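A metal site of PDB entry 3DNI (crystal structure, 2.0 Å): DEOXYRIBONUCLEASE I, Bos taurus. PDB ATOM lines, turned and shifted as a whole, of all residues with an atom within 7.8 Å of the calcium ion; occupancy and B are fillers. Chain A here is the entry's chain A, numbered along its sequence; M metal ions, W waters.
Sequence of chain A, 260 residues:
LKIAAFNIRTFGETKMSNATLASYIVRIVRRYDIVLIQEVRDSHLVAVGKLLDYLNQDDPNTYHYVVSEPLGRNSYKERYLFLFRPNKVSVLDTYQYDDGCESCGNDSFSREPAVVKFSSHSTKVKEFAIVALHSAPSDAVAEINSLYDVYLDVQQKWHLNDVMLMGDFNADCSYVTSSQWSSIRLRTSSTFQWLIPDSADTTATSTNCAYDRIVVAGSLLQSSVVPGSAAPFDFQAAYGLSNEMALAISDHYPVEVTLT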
ATOM      1  N   ALA A 200       4.213   1.592   2.282  1.00  0.00           N
ATOM      2  CA  ALA A 200       2.816   1.792   2.819  1.00  0.00           C
ATOM      3  C   ALA A 200       1.782   1.119   1.915  1.00  0.00           C
ATOM      4  O   ALA A 200       2.069   0.952   0.738  1.00  0.00           O
ATOM      5  CB  ALA A 200       2.551   3.257   3.016  1.00  0.00           C
ATOM      6  N   ASP A 201       0.653   0.739   2.500  1.00  0.00           N
ATOM      7  CA  ASP A 201      -0.447   0.073   1.690  1.00  0.00           C
ATOM      8  C   ASP A 201      -1.585   1.082   1.637  1.00  0.00           C
ATOM      9  O   ASP A 201      -2.305   1.358   2.643  1.00  0.00           O
ATOM     10  CB  ASP A 201      -0.707  -1.291   2.319  1.00  0.00           C
ATOM     11  CG  ASP A 201      -1.931  -1.964   1.589  1.00  0.00           C
ATOM     12  OD1 ASP A 201      -2.254  -1.521   0.469  1.00  0.00           O
ATOM     13  OD2 ASP A 201      -2.436  -2.872   2.202  1.00  0.00           O
ATOM     14  N   THR A 202      -1.858   1.687   0.472  1.00  0.00           N
ATOM     15  CA  THR A 202      -2.969   2.666   0.423  1.00  0.00           C
ATOM     16  C   THR A 202      -4.148   2.071  -0.345  1.00  0.00           C
ATOM     17  O   THR A 202      -4.925   2.886  -0.819  1.00  0.00           O
ATOM     18  CB  THR A 202      -2.441   4.002  -0.214  1.00  0.00           C
ATOM     19  OG1 THR A 202      -2.369   3.741  -1.626  1.00  0.00           O
ATOM     20  CG2 THR A 202      -1.093   4.373   0.476  1.00  0.00           C
ATOM     21  N   THR A 203      -4.227   0.793  -0.550  1.00  0.00           N
ATOM     22  CA  THR A 203      -5.395   0.253  -1.289  1.00  0.00           C
ATOM     23  C   THR A 203      -6.258  -0.597  -0.351  1.00  0.00           C
ATOM     24  O   THR A 203      -5.739  -1.354   0.463  1.00  0.00           O
ATOM     25  CB  THR A 203      -5.001  -0.605  -2.540  1.00  0.00           C
ATOM     26  OG1 THR A 203      -4.573  -1.907  -1.982  1.00  0.00           O
ATOM     27  CG2 THR A 203      -3.911  -0.046  -3.434  1.00  0.00           C
ATOM     28  N   ALA A 204      -7.557  -0.392  -0.493  1.00  0.00           N
ATOM     29  CA  ALA A 204      -8.575  -1.215   0.285  1.00  0.00           C
ATOM     30  C   ALA A 204      -8.604  -2.628  -0.223  1.00  0.00           C
ATOM     31  O   ALA A 204      -8.946  -3.486   0.647  1.00  0.00           O
ATOM     32  CB  ALA A 204      -9.916  -0.502   0.330  1.00  0.00           C
ATOM     33  N   THR A 205      -8.260  -3.018  -1.421  1.00  0.00           N
ATOM     34  CA  THR A 205      -8.230  -4.438  -1.879  1.00  0.00           C
ATOM     35  C   THR A 205      -7.097  -5.259  -1.352  1.00  0.00           C
ATOM     36  O   THR A 205      -6.239  -4.772  -0.514  1.00  0.00           O
ATOM     37  CB  THR A 205      -8.067  -4.338  -3.449  1.00  0.00           C
ATOM     38  OG1 THR A 205      -6.743  -3.743  -3.596  1.00  0.00           O
ATOM     39  CG2 THR A 205      -9.139  -3.442  -4.127  1.00  0.00           C
ATOM     40  N   SER A 206      -6.885  -6.481  -1.788  1.00  0.00           N
ATOM     41  CA  SER A 206      -5.799  -7.365  -1.296  1.00  0.00           C
ATOM     42  C   SER A 206      -4.405  -7.024  -1.766  1.00  0.00           C
ATOM     43  O   SER A 206      -3.446  -7.679  -1.241  1.00  0.00           O
ATOM     44  CB  SER A 206      -6.036  -8.880  -1.569  1.00  0.00           C
ATOM     45  OG  SER A 206      -5.899  -9.024  -2.956  1.00  0.00           O
ATOM     46  N   THR A 207      -4.228  -6.064  -2.667  1.00  0.00           N
ATOM     47  CA  THR A 207      -2.884  -5.717  -3.156  1.00  0.00           C
ATOM     48  C   THR A 207      -2.121  -4.943  -2.094  1.00  0.00           C
ATOM     49  O   THR A 207      -2.806  -4.433  -1.207  1.00  0.00           O
ATOM     50  CB  THR A 207      -2.996  -4.881  -4.497  1.00  0.00           C
ATOM     51  OG1 THR A 207      -3.664  -3.642  -4.152  1.00  0.00           O
ATOM     52  CG2 THR A 207      -3.821  -5.641  -5.538  1.00  0.00           C
ATOM     53  N   ASN A 208      -0.822  -4.849  -2.152  1.00  0.00           N
ATOM     54  CA  ASN A 208      -0.074  -4.078  -1.109  1.00  0.00           C
ATOM     55  C   ASN A 208       0.731  -3.075  -1.942  1.00  0.00           C
ATOM     56  O   ASN A 208       1.851  -3.390  -2.359  1.00  0.00           O
ATOM     57  CB  ASN A 208       0.636  -5.039  -0.185  1.00  0.00           C
ATOM     58  CG  ASN A 208       1.354  -4.411   1.000  1.00  0.00           C
ATOM     59  OD1 ASN A 208       1.843  -3.282   0.875  1.00  0.00           O
ATOM     60  ND2 ASN A 208       1.387  -5.104   2.134  1.00  0.00           N
ATOM     61  N   CYS A 209       0.146  -1.925  -2.175  1.00  0.00           N
ATOM     62  CA  CYS A 209       0.745  -0.900  -3.052  1.00  0.00           C
ATOM     63  C   CYS A 209       0.619   0.487  -2.490  1.00  0.00           C
ATOM     64  O   CYS A 209      -0.477   0.806  -2.012  1.00  0.00           O
ATOM     65  CB  CYS A 209       0.031  -0.925  -4.436  1.00  0.00           C
ATOM     66  SG  CYS A 209       0.045  -2.429  -5.286  1.00  0.00           S
ATOM     67  N   ASP A 234      -7.055   3.390   7.198  1.00  0.00           N
ATOM     68  CA  ASP A 234      -7.723   2.135   6.940  1.00  0.00           C
ATOM     69  C   ASP A 234      -9.107   2.217   7.611  1.00  0.00           C
ATOM     70  O   ASP A 234      -9.189   1.936   8.834  1.00  0.00           O
ATOM     71  CB  ASP A 234      -6.987   0.909   7.476  1.00  0.00           C
ATOM     72  CG  ASP A 234      -7.608  -0.413   7.105  1.00  0.00           C
ATOM     73  OD1 ASP A 234      -8.770  -0.586   6.692  1.00  0.00           O
ATOM     74  OD2 ASP A 234      -6.874  -1.416   7.313  1.00  0.00           O
ATOM     75  N   ASP A 251     -11.700   1.460  -3.364  1.00  0.00           N
ATOM     76  CA  ASP A 251     -10.643   0.461  -3.390  1.00  0.00           C
ATOM     77  C   ASP A 251      -9.311   1.102  -2.904  1.00  0.00           C
ATOM     78  O   ASP A 251      -8.315   0.391  -2.911  1.00  0.00           O
ATOM     79  CB  ASP A 251     -10.479  -0.252  -4.729  1.00  0.00           C
ATOM     80  CG  ASP A 251     -10.298   0.821  -5.826  1.00  0.00           C
ATOM     81  OD1 ASP A 251     -10.713   1.968  -5.742  1.00  0.00           O
ATOM     82  OD2 ASP A 251      -9.779   0.349  -6.813  1.00  0.00           O
ATOM     83  N   TYR A 253      -7.492   3.686   0.256  1.00  0.00           N
ATOM     84  CA  TYR A 253      -7.625   4.367   1.548  1.00  0.00           C
ATOM     85  C   TYR A 253      -7.234   5.845   1.340  1.00  0.00           C
ATOM     86  O   TYR A 253      -6.440   6.196   0.422  1.00  0.00           O
ATOM     87  CB  TYR A 253      -6.642   3.831   2.641  1.00  0.00           C
ATOM     88  CG  TYR A 253      -6.831   2.372   2.916  1.00  0.00           C
ATOM     89  CD1 TYR A 253      -8.140   1.832   3.164  1.00  0.00           C
ATOM     90  CD2 TYR A 253      -5.751   1.540   3.050  1.00  0.00           C
ATOM     91  CE1 TYR A 253      -8.295   0.512   3.533  1.00  0.00           C
ATOM     92  CE2 TYR A 253      -5.876   0.171   3.356  1.00  0.00           C
ATOM     93  CZ  TYR A 253      -7.190  -0.320   3.595  1.00  0.00           C
ATOM     94  OH  TYR A 253      -7.285  -1.650   3.891  1.00  0.00           O
HETATM   95 CA    CA M   1      -4.112  -3.277   0.536  1.00  0.00          CA
HETATM   96  O   HOH W   1      -5.607  -3.663   2.642  1.00  0.00           O
HETATM   97  O   HOH W   2      -3.491  -5.795   1.372  1.00  0.00           O
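Within 4 Å of the calcium ion: Asp 201, Thr 203, Thr 205 and Thr 207.
The nearest printed residue that does not touch the calcium ion is Ser 206 (4.4 Å).
The calcium ion is bound by OD2 of Asp 201, O of Thr 207, O of Thr 203, OD1 of Asp 201, water W1, water W2 and O of Thr 205.
The calcium ion has seven donor atoms within binding distance.
Slightly farther from the calcium ion lies the side-chain hydroxyl (OG1) of Thr 203 (2.9 Å).
The side-chain hydroxyl of Thr 207 lies within hydrogen-bond range of the side-chain hydroxyl of Thr 203 (2.9 Å).
The side-chain hydroxyl (OG1) of Thr 203 is in hydrogen-bond range of the side-chain hydroxyl (OG1) of Thr 205, 3.3 Å away.
The side-chain hydroxyl (OG1) of Thr 207 is in hydrogen-bond range of the side-chain hydroxyl (OG1) of Thr 205.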
